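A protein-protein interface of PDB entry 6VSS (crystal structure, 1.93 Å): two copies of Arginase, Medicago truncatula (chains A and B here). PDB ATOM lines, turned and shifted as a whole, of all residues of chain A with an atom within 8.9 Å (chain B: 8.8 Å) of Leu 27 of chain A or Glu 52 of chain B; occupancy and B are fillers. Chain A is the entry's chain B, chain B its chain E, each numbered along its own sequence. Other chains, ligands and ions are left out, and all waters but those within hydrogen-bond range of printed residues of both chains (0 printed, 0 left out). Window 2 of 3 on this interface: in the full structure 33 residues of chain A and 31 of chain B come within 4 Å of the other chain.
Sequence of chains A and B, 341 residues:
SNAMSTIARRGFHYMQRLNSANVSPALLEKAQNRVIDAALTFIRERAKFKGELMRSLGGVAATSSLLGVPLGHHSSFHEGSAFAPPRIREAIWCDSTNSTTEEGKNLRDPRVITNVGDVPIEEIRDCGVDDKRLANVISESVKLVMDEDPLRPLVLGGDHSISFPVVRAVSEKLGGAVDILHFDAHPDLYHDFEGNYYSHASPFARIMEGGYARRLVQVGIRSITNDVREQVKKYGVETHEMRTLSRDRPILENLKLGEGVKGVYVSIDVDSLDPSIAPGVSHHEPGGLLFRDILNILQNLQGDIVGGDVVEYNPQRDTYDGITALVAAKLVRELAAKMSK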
ATOM      1  N   VAL A  23     -10.930   4.723   7.965  1.00  0.00           N
ATOM      2  CA  VAL A  23     -11.952   5.777   7.762  1.00  0.00           C
ATOM      3  C   VAL A  23     -11.932   6.205   6.285  1.00  0.00           C
ATOM      4  O   VAL A  23     -11.039   7.004   5.920  1.00  0.00           O
ATOM      5  CB  VAL A  23     -11.707   6.979   8.698  1.00  0.00           C
ATOM      6  CG1 VAL A  23     -12.656   8.136   8.398  1.00  0.00           C
ATOM      7  CG2 VAL A  23     -11.774   6.587  10.174  1.00  0.00           C
ATOM      8  N   SER A  24     -12.891   5.715   5.479  1.00  0.00           N
ATOM      9  CA  SER A  24     -13.216   6.234   4.122  1.00  0.00           C
ATOM     10  C   SER A  24     -13.116   7.759   4.123  1.00  0.00           C
ATOM     11  O   SER A  24     -13.701   8.437   4.977  1.00  0.00           O
ATOM     12  CB  SER A  24     -14.578   5.787   3.617  1.00  0.00           C
ATOM     13  OG  SER A  24     -14.767   6.205   2.257  1.00  0.00           O
ATOM     14  N   PRO A  25     -12.362   8.349   3.165  1.00  0.00           N
ATOM     15  CA  PRO A  25     -12.291   9.810   3.041  1.00  0.00           C
ATOM     16  C   PRO A  25     -13.602  10.456   2.534  1.00  0.00           C
ATOM     17  O   PRO A  25     -13.904  11.562   2.978  1.00  0.00           O
ATOM     18  CB  PRO A  25     -11.123  10.056   2.062  1.00  0.00           C
ATOM     19  CG  PRO A  25     -10.526   8.677   1.740  1.00  0.00           C
ATOM     20  CD  PRO A  25     -11.539   7.642   2.176  1.00  0.00           C
ATOM     21  N   ALA A  26     -14.310   9.766   1.618  1.00  0.00           N
ATOM     22  CA  ALA A  26     -15.704  10.008   1.170  1.00  0.00           C
ATOM     23  C   ALA A  26     -16.636  10.340   2.352  1.00  0.00           C
ATOM     24  O   ALA A  26     -17.183  11.465   2.388  1.00  0.00           O
ATOM     25  CB  ALA A  26     -16.219   8.784   0.443  1.00  0.00           C
ATOM     26  N   LEU A  27     -16.798   9.393   3.267  1.00  0.00           N
ATOM     27  CA  LEU A  27     -17.761   9.551   4.382  1.00  0.00           C
ATOM     28  C   LEU A  27     -17.404  10.780   5.217  1.00  0.00           C
ATOM     29  O   LEU A  27     -18.286  11.568   5.472  1.00  0.00           O
ATOM     30  CB  LEU A  27     -17.690   8.285   5.240  1.00  0.00           C
ATOM     31  CG  LEU A  27     -18.658   8.231   6.419  1.00  0.00           C
ATOM     32  CD1 LEU A  27     -19.126   6.809   6.647  1.00  0.00           C
ATOM     33  CD2 LEU A  27     -18.001   8.761   7.669  1.00  0.00           C
ATOM     34  N   LEU A  28     -16.123  10.964   5.500  1.00  0.00           N
ATOM     35  CA  LEU A  28     -15.617  12.063   6.368  1.00  0.00           C
ATOM     36  C   LEU A  28     -15.896  13.420   5.696  1.00  0.00           C
ATOM     37  O   LEU A  28     -16.404  14.322   6.405  1.00  0.00           O
ATOM     38  CB  LEU A  28     -14.125  11.836   6.621  1.00  0.00           C
ATOM     39  CG  LEU A  28     -13.588  12.362   7.947  1.00  0.00           C
ATOM     40  CD1 LEU A  28     -14.025  11.470   9.105  1.00  0.00           C
ATOM     41  CD2 LEU A  28     -12.062  12.475   7.904  1.00  0.00           C
ATOM     42  N   GLU A  29     -15.659  13.511   4.383  1.00  0.00           N
ATOM     43  CA  GLU A  29     -15.853  14.761   3.599  1.00  0.00           C
ATOM     44  C   GLU A  29     -17.325  15.184   3.652  1.00  0.00           C
ATOM     45  O   GLU A  29     -17.589  16.379   3.854  1.00  0.00           O
ATOM     46  CB  GLU A  29     -15.494  14.503   2.132  1.00  0.00           C
ATOM     47  CG  GLU A  29     -16.712  14.388   1.224  1.00  0.00           C
ATOM     48  CD  GLU A  29     -16.603  13.510  -0.011  1.00  0.00           C
ATOM     49  OE1 GLU A  29     -15.637  13.682  -0.783  1.00  0.00           O
ATOM     50  OE2 GLU A  29     -17.497  12.664  -0.202  1.00  0.00           O
ATOM     51  N   LYS A  30     -18.238  14.223   3.494  1.00  0.00           N
ATOM     52  CA  LYS A  30     -19.692  14.512   3.484  1.00  0.00           C
ATOM     53  C   LYS A  30     -20.146  14.817   4.918  1.00  0.00           C
ATOM     54  O   LYS A  30     -20.967  15.709   5.085  1.00  0.00           O
ATOM     55  CB  LYS A  30     -20.436  13.316   2.893  1.00  0.00           C
ATOM     56  CG  LYS A  30     -21.863  13.591   2.444  1.00  0.00           C
ATOM     57  CD  LYS A  30     -22.736  12.347   2.411  1.00  0.00           C
ATOM     58  CE  LYS A  30     -22.670  11.551   3.701  1.00  0.00           C
ATOM     59  NZ  LYS A  30     -23.901  10.763   3.946  1.00  0.00           N
ATOM     60  N   ALA A  31     -19.618  14.130   5.931  1.00  0.00           N
ATOM     61  CA  ALA A  31     -19.897  14.492   7.341  1.00  0.00           C
ATOM     62  C   ALA A  31     -19.550  15.972   7.530  1.00  0.00           C
ATOM     63  O   ALA A  31     -20.428  16.731   8.006  1.00  0.00           O
ATOM     64  CB  ALA A  31     -19.151  13.612   8.314  1.00  0.00           C
ATOM     65  N   GLN A  32     -18.334  16.356   7.128  1.00  0.00           N
ATOM     66  CA  GLN A  32     -17.784  17.730   7.231  1.00  0.00           C
ATOM     67  C   GLN A  32     -18.794  18.743   6.648  1.00  0.00           C
ATOM     68  O   GLN A  32     -19.289  19.557   7.410  1.00  0.00           O
ATOM     69  CB  GLN A  32     -16.376  17.775   6.609  1.00  0.00           C
ATOM     70  CG  GLN A  32     -15.338  16.984   7.399  1.00  0.00           C
ATOM     71  CD  GLN A  32     -13.962  16.891   6.772  1.00  0.00           C
ATOM     72  OE1 GLN A  32     -13.462  17.818   6.128  1.00  0.00           O
ATOM     73  NE2 GLN A  32     -13.279  15.794   7.052  1.00  0.00           N
ATOM     74  N   ASN A  33     -19.117  18.690   5.359  1.00  0.00           N
ATOM     75  CA  ASN A  33     -20.030  19.646   4.684  1.00  0.00           C
ATOM     76  C   ASN A  33     -21.354  19.798   5.435  1.00  0.00           C
ATOM     77  O   ASN A  33     -21.810  20.941   5.652  1.00  0.00           O
ATOM     78  CB  ASN A  33     -20.344  19.205   3.254  1.00  0.00           C
ATOM     79  CG  ASN A  33     -19.084  19.139   2.432  1.00  0.00           C
ATOM     80  OD1 ASN A  33     -18.119  19.827   2.737  1.00  0.00           O
ATOM     81  ND2 ASN A  33     -19.076  18.340   1.391  1.00  0.00           N
ATOM     82  N   ARG A  34     -21.965  18.669   5.771  1.00  0.00           N
ATOM     83  CA  ARG A  34     -23.314  18.581   6.373  1.00  0.00           C
ATOM     84  C   ARG A  34     -23.283  19.183   7.790  1.00  0.00           C
ATOM     85  O   ARG A  34     -24.224  19.972   8.184  1.00  0.00           O
ATOM     86  CB  ARG A  34     -23.731  17.101   6.375  1.00  0.00           C
ATOM     87  CG  ARG A  34     -23.699  16.427   5.006  1.00  0.00           C
ATOM     88  CD  ARG A  34     -24.613  15.218   4.831  1.00  0.00           C
ATOM     89  NE  ARG A  34     -26.030  15.408   5.198  1.00  0.00           N
ATOM     90  CZ  ARG A  34     -26.999  15.847   4.401  1.00  0.00           C
ATOM     91  NH1 ARG A  34     -26.768  16.148   3.131  1.00  0.00           N
ATOM     92  NH2 ARG A  34     -28.222  15.977   4.887  1.00  0.00           N
ATOM     93  N   VAL A  35     -22.272  18.830   8.570  1.00  0.00           N
ATOM     94  CA  VAL A  35     -22.246  19.300   9.997  1.00  0.00           C
ATOM     95  C   VAL A  35     -21.962  20.811  10.002  1.00  0.00           C
ATOM     96  O   VAL A  35     -22.515  21.531  10.814  1.00  0.00           O
ATOM     97  CB  VAL A  35     -21.264  18.515  10.877  1.00  0.00           C
ATOM     98  CG1 VAL A  35     -21.099  19.198  12.238  1.00  0.00           C
ATOM     99  CG2 VAL A  35     -21.724  17.066  11.058  1.00  0.00           C
ATOM    100  N   CYS A 127     -15.217  16.147  13.167  1.00  0.00           N
ATOM    101  CA  CYS A 127     -15.566  15.615  11.815  1.00  0.00           C
ATOM    102  C   CYS A 127     -14.316  15.532  10.941  1.00  0.00           C
ATOM    103  O   CYS A 127     -14.443  15.199   9.738  1.00  0.00           O
ATOM    104  CB  CYS A 127     -16.521  16.523  11.064  1.00  0.00           C
ATOM    105  SG  CYS A 127     -18.095  16.652  11.912  1.00  0.00           S
ATOM    106  N   ARG B  44     -28.856  15.712  14.466  1.00  0.00           N
ATOM    107  CA  ARG B  44     -29.214  14.705  13.446  1.00  0.00           C
ATOM    108  C   ARG B  44     -27.984  14.434  12.575  1.00  0.00           C
ATOM    109  O   ARG B  44     -27.603  13.253  12.430  1.00  0.00           O
ATOM    110  CB  ARG B  44     -30.421  15.155  12.627  1.00  0.00           C
ATOM    111  CG  ARG B  44     -30.811  14.133  11.568  1.00  0.00           C
ATOM    112  CD  ARG B  44     -32.173  14.286  10.912  1.00  0.00           C
ATOM    113  NE  ARG B  44     -32.387  13.157   9.989  1.00  0.00           N
ATOM    114  CZ  ARG B  44     -32.657  11.874  10.339  1.00  0.00           C
ATOM    115  NH1 ARG B  44     -32.779  11.517  11.612  1.00  0.00           N
ATOM    116  NH2 ARG B  44     -32.823  10.937   9.412  1.00  0.00           N
ATOM    117  N   GLU B  45     -27.361  15.473  12.036  1.00  0.00           N
ATOM    118  CA  GLU B  45     -26.206  15.335  11.114  1.00  0.00           C
ATOM    119  C   GLU B  45     -25.040  14.705  11.887  1.00  0.00           C
ATOM    120  O   GLU B  45     -24.330  13.820  11.312  1.00  0.00           O
ATOM    121  CB  GLU B  45     -25.924  16.690  10.483  1.00  0.00           C
ATOM    122  CG  GLU B  45     -27.000  17.157   9.505  1.00  0.00           C
ATOM    123  CD  GLU B  45     -27.240  16.228   8.310  1.00  0.00           C
ATOM    124  OE1 GLU B  45     -26.376  15.347   7.998  1.00  0.00           O
ATOM    125  OE2 GLU B  45     -28.299  16.371   7.695  1.00  0.00           O
ATOM    126  N   ARG B  46     -24.873  15.048  13.180  1.00  0.00           N
ATOM    127  CA  ARG B  46     -23.793  14.439  14.003  1.00  0.00           C
ATOM    128  C   ARG B  46     -24.106  12.959  14.238  1.00  0.00           C
ATOM    129  O   ARG B  46     -23.203  12.117  14.056  1.00  0.00           O
ATOM    130  CB  ARG B  46     -23.566  15.216  15.303  1.00  0.00           C
ATOM    131  CG  ARG B  46     -22.916  16.578  15.073  1.00  0.00           C
ATOM    132  CD  ARG B  46     -21.448  16.543  14.744  1.00  0.00           C
ATOM    133  NE  ARG B  46     -20.781  15.971  15.892  1.00  0.00           N
ATOM    134  CZ  ARG B  46     -19.549  15.483  15.904  1.00  0.00           C
ATOM    135  NH1 ARG B  46     -18.808  15.458  14.815  1.00  0.00           N
ATOM    136  NH2 ARG B  46     -19.056  14.997  17.026  1.00  0.00           N
ATOM    137  N   ALA B  47     -25.330  12.626  14.625  1.00  0.00           N
ATOM    138  CA  ALA B  47     -25.714  11.223  14.854  1.00  0.00           C
ATOM    139  C   ALA B  47     -25.625  10.437  13.524  1.00  0.00           C
ATOM    140  O   ALA B  47     -25.094   9.305  13.535  1.00  0.00           O
ATOM    141  CB  ALA B  47     -27.057  11.182  15.482  1.00  0.00           C
ATOM    142  N   LYS B  48     -26.087  11.020  12.420  1.00  0.00           N
ATOM    143  CA  LYS B  48     -26.026  10.423  11.059  1.00  0.00           C
ATOM    144  C   LYS B  48     -24.564  10.150  10.722  1.00  0.00           C
ATOM    145  O   LYS B  48     -24.267   9.016  10.303  1.00  0.00           O
ATOM    146  CB  LYS B  48     -26.689  11.356  10.039  1.00  0.00           C
ATOM    147  CG  LYS B  48     -26.741  10.837   8.599  1.00  0.00           C
ATOM    148  CD  LYS B  48     -26.514  11.897   7.507  1.00  0.00           C
ATOM    149  CE  LYS B  48     -25.416  11.568   6.497  1.00  0.00           C
ATOM    150  NZ  LYS B  48     -24.063  12.099   6.859  1.00  0.00           N
ATOM    151  N   PHE B  49     -23.660  11.099  11.009  1.00  0.00           N
ATOM    152  CA  PHE B  49     -22.199  10.895  10.796  1.00  0.00           C
ATOM    153  C   PHE B  49     -21.736   9.640  11.568  1.00  0.00           C
ATOM    154  O   PHE B  49     -21.239   8.669  10.930  1.00  0.00           O
ATOM    155  CB  PHE B  49     -21.415  12.185  11.085  1.00  0.00           C
ATOM    156  CG  PHE B  49     -19.919  12.019  11.215  1.00  0.00           C
ATOM    157  CD1 PHE B  49     -19.210  11.154  10.384  1.00  0.00           C
ATOM    158  CD2 PHE B  49     -19.211  12.724  12.183  1.00  0.00           C
ATOM    159  CE1 PHE B  49     -17.836  11.021  10.516  1.00  0.00           C
ATOM    160  CE2 PHE B  49     -17.838  12.571  12.330  1.00  0.00           C
ATOM    161  CZ  PHE B  49     -17.155  11.715  11.498  1.00  0.00           C
ATOM    162  N   LYS B  50     -21.894   9.615  12.888  1.00  0.00           N
ATOM    163  CA  LYS B  50     -21.272   8.581  13.748  1.00  0.00           C
ATOM    164  C   LYS B  50     -21.884   7.217  13.430  1.00  0.00           C
ATOM    165  O   LYS B  50     -21.126   6.223  13.469  1.00  0.00           O
ATOM    166  CB  LYS B  50     -21.404   8.956  15.232  1.00  0.00           C
ATOM    167  CG  LYS B  50     -20.627  10.198  15.629  1.00  0.00           C
ATOM    168  CD  LYS B  50     -19.156  10.109  15.256  1.00  0.00           C
ATOM    169  CE  LYS B  50     -18.363  11.378  15.377  1.00  0.00           C
ATOM    170  NZ  LYS B  50     -18.072  11.657  16.790  1.00  0.00           N
ATOM    171  N   GLY B  51     -23.194   7.144  13.175  1.00  0.00           N
ATOM    172  CA  GLY B  51     -23.850   5.902  12.743  1.00  0.00           C
ATOM    173  C   GLY B  51     -23.084   5.310  11.554  1.00  0.00           C
ATOM    174  O   GLY B  51     -22.517   4.216  11.707  1.00  0.00           O
ATOM    175  N   GLU B  52     -22.967   6.076  10.468  1.00  0.00           N
ATOM    176  CA  GLU B  52     -22.321   5.647   9.199  1.00  0.00           C
ATOM    177  C   GLU B  52     -20.896   5.195   9.503  1.00  0.00           C
ATOM    178  O   GLU B  52     -20.458   4.199   8.886  1.00  0.00           O
ATOM    179  CB  GLU B  52     -22.292   6.778   8.167  1.00  0.00           C
ATOM    180  CG  GLU B  52     -23.501   6.797   7.243  1.00  0.00           C
ATOM    181  CD  GLU B  52     -23.626   8.016   6.333  1.00  0.00           C
ATOM    182  OE1 GLU B  52     -22.579   8.527   5.885  1.00  0.00           O
ATOM    183  OE2 GLU B  52     -24.778   8.476   6.090  1.00  0.00           O
ATOM    184  N   LEU B  53     -20.201   5.911  10.404  1.00  0.00           N
ATOM    185  CA  LEU B  53     -18.801   5.585  10.798  1.00  0.00           C
ATOM    186  C   LEU B  53     -18.810   4.174  11.403  1.00  0.00           C
ATOM    187  O   LEU B  53     -18.100   3.316  10.844  1.00  0.00           O
ATOM    188  CB  LEU B  53     -18.194   6.656  11.723  1.00  0.00           C
ATOM    189  CG  LEU B  53     -16.758   6.416  12.224  1.00  0.00           C
ATOM    190  CD1 LEU B  53     -15.756   6.313  11.081  1.00  0.00           C
ATOM    191  CD2 LEU B  53     -16.290   7.496  13.200  1.00  0.00           C
ATOM    192  N   MET B  54     -19.658   3.888  12.390  1.00  0.00           N
ATOM    193  CA  MET B  54     -19.619   2.553  13.040  1.00  0.00           C
ATOM    194  C   MET B  54     -19.994   1.458  12.022  1.00  0.00           C
ATOM    195  O   MET B  54     -19.250   0.440  11.936  1.00  0.00           O
ATOM    196  CB  MET B  54     -20.502   2.475  14.294  1.00  0.00           C
ATOM    197  CG  MET B  54     -20.140   3.510  15.376  1.00  0.00           C
ATOM    198  SD  MET B  54     -18.391   4.052  15.420  1.00  0.00           S
ATOM    199  CE  MET B  54     -18.659   5.659  16.163  1.00  0.00           C
ATOM    200  N   ARG B  55     -21.078   1.663  11.273  1.00  0.00           N
ATOM    201  CA  ARG B  55     -21.599   0.691  10.272  1.00  0.00           C
ATOM    202  C   ARG B  55     -20.500   0.423   9.227  1.00  0.00           C
ATOM    203  O   ARG B  55     -20.228  -0.730   8.967  1.00  0.00           O
ATOM    204  CB  ARG B  55     -22.920   1.183   9.666  1.00  0.00           C
ATOM    205  CG  ARG B  55     -24.099   1.094  10.628  1.00  0.00           C
ATOM    206  CD  ARG B  55     -25.426   1.366   9.977  1.00  0.00           C
ATOM    207  NE  ARG B  55     -25.347   2.495   9.069  1.00  0.00           N
ATOM    208  CZ  ARG B  55     -25.779   3.722   9.334  1.00  0.00           C
ATOM    209  NH1 ARG B  55     -26.329   4.017  10.499  1.00  0.00           N
ATOM    210  NH2 ARG B  55     -25.646   4.664   8.427  1.00  0.00           N
ATOM    211  N   SER B  56     -19.809   1.432   8.718  1.00  0.00           N
ATOM    212  CA  SER B  56     -18.719   1.214   7.738  1.00  0.00           C
ATOM    213  C   SER B  56     -17.557   0.449   8.393  1.00  0.00           C
ATOM    214  O   SER B  56     -16.903  -0.309   7.668  1.00  0.00           O
ATOM    215  CB  SER B  56     -18.261   2.496   7.155  1.00  0.00           C
ATOM    216  OG  SER B  56     -17.486   3.145   8.130  1.00  0.00           O
ATOM    217  N   LEU B  57     -17.333   0.608   9.708  1.00  0.00           N
ATOM    218  CA  LEU B  57     -16.190   0.010  10.460  1.00  0.00           C
ATOM    219  C   LEU B  57     -16.466  -1.455  10.784  1.00  0.00           C
ATOM    220  O   LEU B  57     -15.463  -2.199  10.850  1.00  0.00           O
ATOM    221  CB  LEU B  57     -15.912   0.783  11.754  1.00  0.00           C
ATOM    222  CG  LEU B  57     -15.229   2.141  11.573  1.00  0.00           C
ATOM    223  CD1 LEU B  57     -15.102   2.865  12.901  1.00  0.00           C
ATOM    224  CD2 LEU B  57     -13.859   1.988  10.921  1.00  0.00           C
ATOM    225  N   GLY B  58     -17.741  -1.827  11.008  1.00  0.00           N
ATOM    226  CA  GLY B  58     -18.200  -3.202  11.314  1.00  0.00           C
ATOM    227  C   GLY B  58     -17.639  -3.728  12.635  1.00  0.00           C
ATOM    228  O   GLY B  58     -16.952  -2.971  13.310  1.00  0.00           O
ATOM    229  N   VAL B  60     -19.232  -4.308  15.358  1.00  0.00           N
ATOM    230  CA  VAL B  60     -19.940  -3.659  16.503  1.00  0.00           C
ATOM    231  C   VAL B  60     -21.461  -3.852  16.410  1.00  0.00           C
ATOM    232  O   VAL B  60     -22.005  -3.825  15.293  1.00  0.00           O
ATOM    233  CB  VAL B  60     -19.589  -2.160  16.544  1.00  0.00           C
ATOM    234  CG1 VAL B  60     -19.343  -1.608  15.150  1.00  0.00           C
ATOM    235  CG2 VAL B  60     -20.653  -1.347  17.261  1.00  0.00           C
ATOM    236  N   ARG B 111     -15.791   2.659  18.061  1.00  0.00           N
ATOM    237  CA  ARG B 111     -16.923   1.727  18.262  1.00  0.00           C
ATOM    238  C   ARG B 111     -17.175   1.529  19.749  1.00  0.00           C
ATOM    239  O   ARG B 111     -18.273   1.066  20.063  1.00  0.00           O
ATOM    240  CB  ARG B 111     -16.669   0.425  17.514  1.00  0.00           C
ATOM    241  CG  ARG B 111     -16.815   0.598  16.009  1.00  0.00           C
ATOM    242  CD  ARG B 111     -16.253  -0.607  15.294  1.00  0.00           C
ATOM    243  NE  ARG B 111     -14.821  -0.716  15.496  1.00  0.00           N
ATOM    244  CZ  ARG B 111     -14.113  -1.815  15.302  1.00  0.00           C
ATOM    245  NH1 ARG B 111     -14.696  -2.941  14.918  1.00  0.00           N
ATOM    246  NH2 ARG B 111     -12.810  -1.789  15.506  1.00  0.00           N
ATOM    247  N   GLU B 148     -30.055   5.898  14.834  1.00  0.00           N
ATOM    248  CA  GLU B 148     -28.816   5.560  14.088  1.00  0.00           C
ATOM    249  C   GLU B 148     -28.154   4.305  14.674  1.00  0.00           C
ATOM    250  O   GLU B 148     -27.329   4.421  15.625  1.00  0.00           O
ATOM    251  CB  GLU B 148     -27.896   6.772  14.094  1.00  0.00           C
ATOM    252  CG  GLU B 148     -28.391   7.850  13.172  1.00  0.00           C
ATOM    253  CD  GLU B 148     -28.558   7.406  11.724  1.00  0.00           C
ATOM    254  OE1 GLU B 148     -27.943   6.394  11.318  1.00  0.00           O
ATOM    255  OE2 GLU B 148     -29.318   8.059  11.016  1.00  0.00           O
ATOM    256  N   ASP B 149     -28.453   3.140  14.108  1.00  0.00           N
ATOM    257  CA  ASP B 149     -27.766   1.885  14.494  1.00  0.00           C
ATOM    258  C   ASP B 149     -26.269   2.027  14.191  1.00  0.00           C
ATOM    259  O   ASP B 149     -25.865   2.471  13.112  1.00  0.00           O
ATOM    260  CB  ASP B 149     -28.370   0.668  13.788  1.00  0.00           C
ATOM    261  CG  ASP B 149     -27.722  -0.623  14.265  1.00  0.00           C
ATOM    262  OD1 ASP B 149     -27.929  -0.991  15.459  1.00  0.00           O
ATOM    263  OD2 ASP B 149     -26.935  -1.204  13.484  1.00  0.00           O
ATOM    264  N   PRO B 150     -25.368   1.645  15.113  1.00  0.00           N
ATOM    265  CA  PRO B 150     -25.706   1.030  16.393  1.00  0.00           C
ATOM    266  C   PRO B 150     -25.436   1.933  17.606  1.00  0.00           C
ATOM    267  O   PRO B 150     -25.023   1.460  18.641  1.00  0.00           O
ATOM    268  CB  PRO B 150     -24.745  -0.160  16.324  1.00  0.00           C
ATOM    269  CG  PRO B 150     -23.477   0.442  15.736  1.00  0.00           C
ATOM    270  CD  PRO B 150     -23.915   1.651  14.923  1.00  0.00           C
ATOM    271  N   LEU B 151     -25.767   3.199  17.482  1.00  0.00           N
ATOM    272  CA  LEU B 151     -25.557   4.148  18.593  1.00  0.00           C
ATOM    273  C   LEU B 151     -26.560   3.902  19.713  1.00  0.00           C
ATOM    274  O   LEU B 151     -27.741   3.789  19.429  1.00  0.00           O
ATOM    275  CB  LEU B 151     -25.681   5.580  18.086  1.00  0.00           C
ATOM    276  CG  LEU B 151     -24.838   5.945  16.871  1.00  0.00           C
ATOM    277  CD1 LEU B 151     -25.047   7.397  16.577  1.00  0.00           C
ATOM    278  CD2 LEU B 151     -23.353   5.632  17.075  1.00  0.00           C
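Leu 27 of chain A touches Phe 49 of chain B.
CB of Glu 52 of chain B touches CD1 of Leu 27 of chain A, 3.5 Å away.
Leu 28 of chain A touches Phe 49 of chain B.
CD1 of Phe 49 of chain B touches CB of Ala 31 of chain A (3.2 Å).
Lys 48 of chain B touches Arg 34 of chain A (NZ to CD, 3.8 Å).
Val 35 of chain A touches Arg 46 of chain B (CG1 to CD, 3.7 Å).
CA of Cys 127 of chain A touches CE2 of Phe 49 of chain B, at 3.8 Å.
Of the printed residues of chain A, Glu 52 of chain B touches Leu 27 and Lys 30.
No residue of chain B comes within 4 Å of Ala 26 of chain A.
Of the printed residues of chain A, Arg 46 of chain B touches Val 35 (3.7 Å) and Cys 127 (3.2 Å).
Printed residues of chain B within 4 Å of Val 35 of chain A: Arg 46.
Of the printed residues of chain B, Cys 127 of chain A touches Arg 46 and Phe 49.
Printed residues of chain A within 4 Å of Phe 49 of chain B: Leu 27, Leu 28, Ala 31 and Cys 127.
Printed residues of chain A within 4 Å of Lys 48 of chain B: Lys 30 and Arg 34.
Lys 50 of chain B touches none of the printed residues of chain A.
O of Cys 127 of chain A sits at hydrogen-bond distance from NE2 of Gln 32 of chain A (3.0 Å).
The side-chain carboxylate (OE2) of Glu 52 of chain B lies within salt-bridge range of the side-chain amino group (NZ) of Lys 48 of chain B (3.8 Å).
O of Glu 52 of chain B sits at hydrogen-bond distance from OG of Ser 56 of chain B, 3.2 Å away.
The side-chain amino group (NZ) of Lys 30 of chain A lies within salt-bridge range of the side-chain carboxylate (OE1) of Glu 52 of chain B.
NE of Arg 34 of chain A lies within salt-bridge range of OE1 of Glu 45 of chain B, 2.8 Å away.
SG of Cys 127 of chain A is in hydrogen-bond range of NH1 of Arg 46 of chain B, at 3.2 Å.
The side-chain amino group of Lys 48 of chain B sits close to the side-chain amino group of Lys 30 of chain A.
Of the 21 printed residues of chain B, 5 touch a printed residue of chain A.
Printed residues of chain B that touch a printed residue of chain A: Glu 45, Arg 46, Lys 48, Phe 49 and Glu 52.
Of the 14 printed residues of chain A, 7 touch a printed residue of chain B.
Hydrophobic or aromatic side chains of chain A within 4 Å of the printed part of chain B: Leu 27, Leu 28, Ala 31 and Val 35.
Along chain A the printed residues that touch a printed residue of chain B span positions 27 to 127.
No position is printed for both chains.
Of the 11 pairs that touch across the chains among the printed residues, none has its exchanged pair printed and touching as well.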
